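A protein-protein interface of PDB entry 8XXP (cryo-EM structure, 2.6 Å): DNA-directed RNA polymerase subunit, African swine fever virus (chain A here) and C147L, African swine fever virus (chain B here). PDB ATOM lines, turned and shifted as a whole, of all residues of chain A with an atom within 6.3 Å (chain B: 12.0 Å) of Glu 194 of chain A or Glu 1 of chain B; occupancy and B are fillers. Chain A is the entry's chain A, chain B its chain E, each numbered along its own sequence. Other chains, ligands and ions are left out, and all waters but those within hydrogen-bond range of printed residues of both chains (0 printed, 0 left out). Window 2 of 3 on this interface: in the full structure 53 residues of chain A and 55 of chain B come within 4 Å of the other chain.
ND2 of Asn 19 of chain A lies close to O of Ser 2 of chain B.
The side-chain carboxylate of Glu 194 of chain A lies within hydrogen-bond range of the side-chain hydroxyl of Ser 2 of chain B, 2.4 Å away.
NZ of Lys 195 of chain A is in hydrogen-bond range of O of Pro 3 of chain B (3.2 Å).
OE1 of Glu 194 of chain A is in salt-bridge range of NH1 of Arg 171 of chain A, 2.6 Å away.
The backbone NH (N) of Glu 194 of chain A sits close to a ring nitrogen (ND1) of His 192 of chain A (3.3 Å).
The side-chain hydroxyl (OG) of Ser 4 of chain B sits at hydrogen-bond distance from the side-chain sulfur (SG) of Cys 6 of chain B.
The backbone NH (N) of Ser 4 of chain B is in hydrogen-bond range of the side-chain carboxylate (OE2) of Glu 7 of chain B (3.1 Å).
Asn 19 of chain A touches Glu 1 of chain B (ND2 to OE1, 3.9 Å).
Asn 19 of chain A touches Pro 3 of chain B.
Asn 19 of chain A touches Ser 4 of chain B.
Ser 2 of chain B touches Tyr 179 of chain A.
Tyr 179 of chain A touches Pro 3 of chain B (OH to CD, 3.6 Å).
CB of His 192 of chain A touches OG of Ser 2 of chain B (3.6 Å).
Glu 194 of chain A touches Glu 1 of chain B (OE2 to C, 3.6 Å).
Lys 195 of chain A touches Ser 2 of chain B.
Printed residues of chain B within 4 Å of Asn 19 of chain A: Glu 1, Ser 2, Pro 3 and Ser 4.
No residue of chain B comes within 4 Å of Arg 171 of chain A.
No residue of chain B comes within 4 Å of Ser 175 of chain A.
Printed residues of chain B within 4 Å of Tyr 179 of chain A: Ser 2 and Pro 3.
No residue of chain B comes within 4 Å of Pro 193 of chain A.
Glu 194 of chain A touches just these residues of chain B: Glu 1 and Ser 2.
No residue of chain B comes within 4 Å of Leu 196 of chain A.
Glu 1 of chain B touches just these residues of chain A: Asn 19 (3.9 Å) and Glu 194 (3.6 Å).
Printed residues of chain A within 4 Å of Ser 2 of chain B: Asn 19, Tyr 179, His 192, Glu 194 and Lys 195.
Of the printed residues of chain A, Pro 3 of chain B touches Asn 19 (3.98 Å), Tyr 179 (3.6 Å) and Lys 195 (3.2 Å).
The nearest residue of chain B that does not touch Glu 194 of chain A is Pro 3 of chain B (5.6 Å).
Of the 15 printed residues of chain A, 5 touch a printed residue of chain B.
Hydrophobic or aromatic side chains of chain A within 4 Å of the printed part of chain B: Tyr 179 and His 192.
Among the printed residues, no Asp or Glu carboxylate lies within 4 Å of a Lys or Arg side-chain nitrogen of the other chain.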
ATOM      1  N   GLY A  17     -17.909 -15.599  -3.930  1.00  0.00           N
ATOM      2  CA  GLY A  17     -17.810 -14.217  -4.337  1.00  0.00           C
ATOM      3  C   GLY A  17     -16.681 -13.976  -5.321  1.00  0.00           C
ATOM      4  O   GLY A  17     -16.110 -14.897  -5.906  1.00  0.00           O
ATOM      5  N   ASN A  19     -13.734 -12.802  -4.549  1.00  0.00           N
ATOM      6  CA  ASN A  19     -12.480 -13.266  -3.971  1.00  0.00           C
ATOM      7  C   ASN A  19     -12.278 -14.751  -4.223  1.00  0.00           C
ATOM      8  O   ASN A  19     -11.156 -15.194  -4.484  1.00  0.00           O
ATOM      9  CB  ASN A  19     -12.451 -12.970  -2.472  1.00  0.00           C
ATOM     10  CG  ASN A  19     -12.252 -11.493  -2.169  1.00  0.00           C
ATOM     11  OD1 ASN A  19     -12.844 -10.629  -2.816  1.00  0.00           O
ATOM     12  ND2 ASN A  19     -11.417 -11.198  -1.180  1.00  0.00           N
ATOM     13  N   ILE A 170     -26.384  -1.890  -6.667  1.00  0.00           N
ATOM     14  CA  ILE A 170     -26.702  -2.927  -5.693  1.00  0.00           C
ATOM     15  C   ILE A 170     -25.448  -3.367  -4.952  1.00  0.00           C
ATOM     16  O   ILE A 170     -25.485  -3.634  -3.746  1.00  0.00           O
ATOM     17  CB  ILE A 170     -27.398  -4.104  -6.397  1.00  0.00           C
ATOM     18  CG1 ILE A 170     -28.634  -3.608  -7.141  1.00  0.00           C
ATOM     19  CG2 ILE A 170     -27.798  -5.154  -5.408  1.00  0.00           C
ATOM     20  CD1 ILE A 170     -29.295  -4.656  -7.986  1.00  0.00           C
ATOM     21  N   ARG A 171     -24.316  -3.438  -5.655  1.00  0.00           N
ATOM     22  CA  ARG A 171     -23.063  -3.806  -5.008  1.00  0.00           C
ATOM     23  C   ARG A 171     -22.661  -2.780  -3.960  1.00  0.00           C
ATOM     24  O   ARG A 171     -22.236  -3.144  -2.861  1.00  0.00           O
ATOM     25  CB  ARG A 171     -21.956  -3.966  -6.048  1.00  0.00           C
ATOM     26  CG  ARG A 171     -20.555  -3.774  -5.492  1.00  0.00           C
ATOM     27  CD  ARG A 171     -20.050  -5.033  -4.821  1.00  0.00           C
ATOM     28  NE  ARG A 171     -19.163  -5.791  -5.692  1.00  0.00           N
ATOM     29  CZ  ARG A 171     -18.224  -6.623  -5.265  1.00  0.00           C
ATOM     30  NH1 ARG A 171     -18.039  -6.854  -3.978  1.00  0.00           N
ATOM     31  NH2 ARG A 171     -17.455  -7.244  -6.154  1.00  0.00           N
ATOM     32  N   PHE A 174     -25.033  -3.124  -0.914  1.00  0.00           N
ATOM     33  CA  PHE A 174     -24.727  -4.280  -0.089  1.00  0.00           C
ATOM     34  C   PHE A 174     -23.359  -4.178   0.561  1.00  0.00           C
ATOM     35  O   PHE A 174     -23.139  -4.791   1.608  1.00  0.00           O
ATOM     36  CB  PHE A 174     -24.826  -5.548  -0.931  1.00  0.00           C
ATOM     37  CG  PHE A 174     -26.228  -5.910  -1.303  1.00  0.00           C
ATOM     38  CD1 PHE A 174     -27.297  -5.373  -0.617  1.00  0.00           C
ATOM     39  CD2 PHE A 174     -26.479  -6.791  -2.335  1.00  0.00           C
ATOM     40  CE1 PHE A 174     -28.590  -5.706  -0.959  1.00  0.00           C
ATOM     41  CE2 PHE A 174     -27.769  -7.130  -2.672  1.00  0.00           C
ATOM     42  CZ  PHE A 174     -28.824  -6.582  -1.988  1.00  0.00           C
ATOM     43  N   SER A 175     -22.434  -3.424  -0.030  1.00  0.00           N
ATOM     44  CA  SER A 175     -21.150  -3.198   0.619  1.00  0.00           C
ATOM     45  C   SER A 175     -21.303  -2.306   1.837  1.00  0.00           C
ATOM     46  O   SER A 175     -20.533  -2.432   2.794  1.00  0.00           O
ATOM     47  CB  SER A 175     -20.160  -2.581  -0.365  1.00  0.00           C
ATOM     48  OG  SER A 175     -18.893  -2.413   0.238  1.00  0.00           O
ATOM     49  N   TYR A 179     -21.489  -6.534   8.982  1.00  0.00           N
ATOM     50  CA  TYR A 179     -21.632  -7.948   9.312  1.00  0.00           C
ATOM     51  C   TYR A 179     -22.618  -8.163  10.450  1.00  0.00           C
ATOM     52  O   TYR A 179     -23.247  -9.223  10.530  1.00  0.00           O
ATOM     53  CB  TYR A 179     -20.276  -8.549   9.673  1.00  0.00           C
ATOM     54  CG  TYR A 179     -19.434  -8.908   8.475  1.00  0.00           C
ATOM     55  CD1 TYR A 179     -19.770  -9.981   7.664  1.00  0.00           C
ATOM     56  CD2 TYR A 179     -18.302  -8.177   8.155  1.00  0.00           C
ATOM     57  CE1 TYR A 179     -19.006 -10.312   6.569  1.00  0.00           C
ATOM     58  CE2 TYR A 179     -17.532  -8.501   7.063  1.00  0.00           C
ATOM     59  CZ  TYR A 179     -17.886  -9.569   6.274  1.00  0.00           C
ATOM     60  OH  TYR A 179     -17.116  -9.895   5.181  1.00  0.00           O
ATOM     61  N   SER A 191     -22.430 -15.442   3.943  1.00  0.00           N
ATOM     62  CA  SER A 191     -23.584 -15.066   3.141  1.00  0.00           C
ATOM     63  C   SER A 191     -23.828 -13.562   3.149  1.00  0.00           C
ATOM     64  O   SER A 191     -24.979 -13.122   3.089  1.00  0.00           O
ATOM     65  CB  SER A 191     -24.825 -15.811   3.626  1.00  0.00           C
ATOM     66  OG  SER A 191     -24.899 -17.096   3.041  1.00  0.00           O
ATOM     67  N   HIS A 192     -22.766 -12.768   3.228  1.00  0.00           N
ATOM     68  CA  HIS A 192     -22.914 -11.325   3.156  1.00  0.00           C
ATOM     69  C   HIS A 192     -23.497 -10.938   1.801  1.00  0.00           C
ATOM     70  O   HIS A 192     -23.074 -11.470   0.770  1.00  0.00           O
ATOM     71  CB  HIS A 192     -21.565 -10.640   3.364  1.00  0.00           C
ATOM     72  CG  HIS A 192     -21.668  -9.192   3.733  1.00  0.00           C
ATOM     73  ND1 HIS A 192     -22.062  -8.221   2.839  1.00  0.00           N
ATOM     74  CD2 HIS A 192     -21.414  -8.550   4.896  1.00  0.00           C
ATOM     75  CE1 HIS A 192     -22.051  -7.044   3.437  1.00  0.00           C
ATOM     76  NE2 HIS A 192     -21.661  -7.215   4.686  1.00  0.00           N
ATOM     77  N   PRO A 193     -24.470 -10.027   1.764  1.00  0.00           N
ATOM     78  CA  PRO A 193     -25.154  -9.737   0.495  1.00  0.00           C
ATOM     79  C   PRO A 193     -24.253  -9.165  -0.584  1.00  0.00           C
ATOM     80  O   PRO A 193     -24.628  -9.210  -1.760  1.00  0.00           O
ATOM     81  CB  PRO A 193     -26.243  -8.740   0.906  1.00  0.00           C
ATOM     82  CG  PRO A 193     -25.766  -8.171   2.198  1.00  0.00           C
ATOM     83  CD  PRO A 193     -25.063  -9.284   2.884  1.00  0.00           C
ATOM     84  N   GLU A 194     -23.086  -8.622  -0.238  1.00  0.00           N
ATOM     85  CA  GLU A 194     -22.214  -8.085  -1.274  1.00  0.00           C
ATOM     86  C   GLU A 194     -21.641  -9.181  -2.159  1.00  0.00           C
ATOM     87  O   GLU A 194     -21.246  -8.899  -3.293  1.00  0.00           O
ATOM     88  CB  GLU A 194     -21.085  -7.260  -0.652  1.00  0.00           C
ATOM     89  CG  GLU A 194     -20.091  -8.060   0.149  1.00  0.00           C
ATOM     90  CD  GLU A 194     -18.859  -8.393  -0.654  1.00  0.00           C
ATOM     91  OE1 GLU A 194     -18.513  -7.611  -1.562  1.00  0.00           O
ATOM     92  OE2 GLU A 194     -18.241  -9.441  -0.394  1.00  0.00           O
ATOM     93  N   LYS A 195     -21.595 -10.423  -1.671  1.00  0.00           N
ATOM     94  CA  LYS A 195     -21.186 -11.553  -2.496  1.00  0.00           C
ATOM     95  C   LYS A 195     -22.146 -11.800  -3.648  1.00  0.00           C
ATOM     96  O   LYS A 195     -21.778 -12.478  -4.611  1.00  0.00           O
ATOM     97  CB  LYS A 195     -21.098 -12.825  -1.654  1.00  0.00           C
ATOM     98  CG  LYS A 195     -19.845 -12.982  -0.810  1.00  0.00           C
ATOM     99  CD  LYS A 195     -19.769 -14.396  -0.254  1.00  0.00           C
ATOM    100  CE  LYS A 195     -18.700 -14.535   0.813  1.00  0.00           C
ATOM    101  NZ  LYS A 195     -17.348 -14.798   0.251  1.00  0.00           N
ATOM    102  N   LEU A 196     -23.366 -11.276  -3.566  1.00  0.00           N
ATOM    103  CA  LEU A 196     -24.395 -11.586  -4.545  1.00  0.00           C
ATOM    104  C   LEU A 196     -24.230 -10.818  -5.845  1.00  0.00           C
ATOM    105  O   LEU A 196     -24.958 -11.097  -6.803  1.00  0.00           O
ATOM    106  CB  LEU A 196     -25.769 -11.310  -3.942  1.00  0.00           C
ATOM    107  CG  LEU A 196     -25.983 -11.962  -2.581  1.00  0.00           C
ATOM    108  CD1 LEU A 196     -27.320 -11.558  -2.000  1.00  0.00           C
ATOM    109  CD2 LEU A 196     -25.880 -13.464  -2.706  1.00  0.00           C
ATOM    110  N   VAL A 197     -23.305  -9.867  -5.902  1.00  0.00           N
ATOM    111  CA  VAL A 197     -22.971  -9.153  -7.128  1.00  0.00           C
ATOM    112  C   VAL A 197     -21.534  -9.497  -7.483  1.00  0.00           C
ATOM    113  O   VAL A 197     -20.613  -9.245  -6.696  1.00  0.00           O
ATOM    114  CB  VAL A 197     -23.153  -7.636  -6.973  1.00  0.00           C
ATOM    115  CG1 VAL A 197     -23.313  -6.989  -8.334  1.00  0.00           C
ATOM    116  CG2 VAL A 197     -24.342  -7.329  -6.079  1.00  0.00           C
ATOM    117  N   LEU A 198     -21.341 -10.062  -8.670  1.00  0.00           N
ATOM    118  CA  LEU A 198     -20.037 -10.519  -9.125  1.00  0.00           C
ATOM    119  C   LEU A 198     -19.470  -9.539 -10.138  1.00  0.00           C
ATOM    120  O   LEU A 198     -20.155  -9.162 -11.090  1.00  0.00           O
ATOM    121  CB  LEU A 198     -20.134 -11.902  -9.763  1.00  0.00           C
ATOM    122  CG  LEU A 198     -20.403 -13.104  -8.874  1.00  0.00           C
ATOM    123  CD1 LEU A 198     -20.465 -14.328  -9.747  1.00  0.00           C
ATOM    124  CD2 LEU A 198     -19.333 -13.251  -7.818  1.00  0.00           C
ATOM    125  N   GLU B   1     -15.698  -5.887   0.993  1.00  0.00           N
ATOM    126  CA  GLU B   1     -15.409  -7.123   0.274  1.00  0.00           C
ATOM    127  C   GLU B   1     -15.263  -8.308   1.225  1.00  0.00           C
ATOM    128  O   GLU B   1     -14.467  -8.272   2.162  1.00  0.00           O
ATOM    129  CB  GLU B   1     -14.147  -6.960  -0.575  1.00  0.00           C
ATOM    130  CG  GLU B   1     -13.098  -6.031   0.024  1.00  0.00           C
ATOM    131  CD  GLU B   1     -12.199  -6.718   1.037  1.00  0.00           C
ATOM    132  OE1 GLU B   1     -11.830  -7.892   0.816  1.00  0.00           O
ATOM    133  OE2 GLU B   1     -11.859  -6.081   2.057  1.00  0.00           O
ATOM    134  N   SER B   2     -16.051  -9.349   0.986  1.00  0.00           N
ATOM    135  CA  SER B   2     -15.965 -10.541   1.812  1.00  0.00           C
ATOM    136  C   SER B   2     -14.698 -11.320   1.474  1.00  0.00           C
ATOM    137  O   SER B   2     -14.282 -11.354   0.313  1.00  0.00           O
ATOM    138  CB  SER B   2     -17.187 -11.433   1.605  1.00  0.00           C
ATOM    139  OG  SER B   2     -18.390 -10.687   1.705  1.00  0.00           O
ATOM    140  N   PRO B   3     -14.061 -11.945   2.457  1.00  0.00           N
ATOM    141  CA  PRO B   3     -12.885 -12.768   2.168  1.00  0.00           C
ATOM    142  C   PRO B   3     -13.295 -14.090   1.545  1.00  0.00           C
ATOM    143  O   PRO B   3     -14.462 -14.483   1.548  1.00  0.00           O
ATOM    144  CB  PRO B   3     -12.252 -12.970   3.544  1.00  0.00           C
ATOM    145  CG  PRO B   3     -13.406 -12.909   4.479  1.00  0.00           C
ATOM    146  CD  PRO B   3     -14.374 -11.918   3.895  1.00  0.00           C
ATOM    147  N   SER B   4     -12.308 -14.780   0.987  1.00  0.00           N
ATOM    148  CA  SER B   4     -12.562 -16.114   0.471  1.00  0.00           C
ATOM    149  C   SER B   4     -12.913 -17.053   1.617  1.00  0.00           C
ATOM    150  O   SER B   4     -12.380 -16.943   2.725  1.00  0.00           O
ATOM    151  CB  SER B   4     -11.346 -16.633  -0.296  1.00  0.00           C
ATOM    152  OG  SER B   4     -11.567 -17.948  -0.773  1.00  0.00           O
ATOM    153  N   ILE B   5     -13.829 -17.984   1.342  1.00  0.00           N
ATOM    154  CA  ILE B   5     -14.277 -18.919   2.368  1.00  0.00           C
ATOM    155  C   ILE B   5     -13.116 -19.769   2.866  1.00  0.00           C
ATOM    156  O   ILE B   5     -13.083 -20.181   4.031  1.00  0.00           O
ATOM    157  CB  ILE B   5     -15.436 -19.781   1.838  1.00  0.00           C
ATOM    158  CG1 ILE B   5     -16.541 -18.879   1.290  1.00  0.00           C
ATOM    159  CG2 ILE B   5     -15.981 -20.680   2.927  1.00  0.00           C
ATOM    160  CD1 ILE B   5     -17.203 -19.411   0.070  1.00  0.00           C
ATOM    161  N   CYS B   6     -12.141 -20.037   1.996  1.00  0.00           N
ATOM    162  CA  CYS B   6     -10.965 -20.793   2.411  1.00  0.00           C
ATOM    163  C   CYS B   6     -10.213 -20.093   3.535  1.00  0.00           C
ATOM    164  O   CYS B   6      -9.563 -20.756   4.351  1.00  0.00           O
ATOM    165  CB  CYS B   6     -10.045 -21.015   1.214  1.00  0.00           C
ATOM    166  SG  CYS B   6      -9.417 -19.500   0.468  1.00  0.00           S
ATOM    167  N   GLU B   7     -10.287 -18.762   3.595  1.00  0.00           N
ATOM    168  CA  GLU B   7      -9.576 -18.026   4.635  1.00  0.00           C
ATOM    169  C   GLU B   7     -10.175 -18.282   6.013  1.00  0.00           C
ATOM    170  O   GLU B   7      -9.442 -18.527   6.977  1.00  0.00           O
ATOM    171  CB  GLU B   7      -9.586 -16.532   4.314  1.00  0.00           C
ATOM    172  CG  GLU B   7      -8.955 -16.189   2.977  1.00  0.00           C
ATOM    173  CD  GLU B   7      -9.088 -14.720   2.628  1.00  0.00           C
ATOM    174  OE1 GLU B   7      -9.036 -13.882   3.552  1.00  0.00           O
ATOM    175  OE2 GLU B   7      -9.239 -14.403   1.430  1.00  0.00           O
ATOM    176  N   GLY B   8     -11.495 -18.229   6.128  1.00  0.00           N
ATOM    177  CA  GLY B   8     -12.157 -18.450   7.393  1.00  0.00           C
ATOM    178  C   GLY B   8     -12.471 -19.889   7.719  1.00  0.00           C
ATOM    179  O   GLY B   8     -13.091 -20.161   8.751  1.00  0.00           O
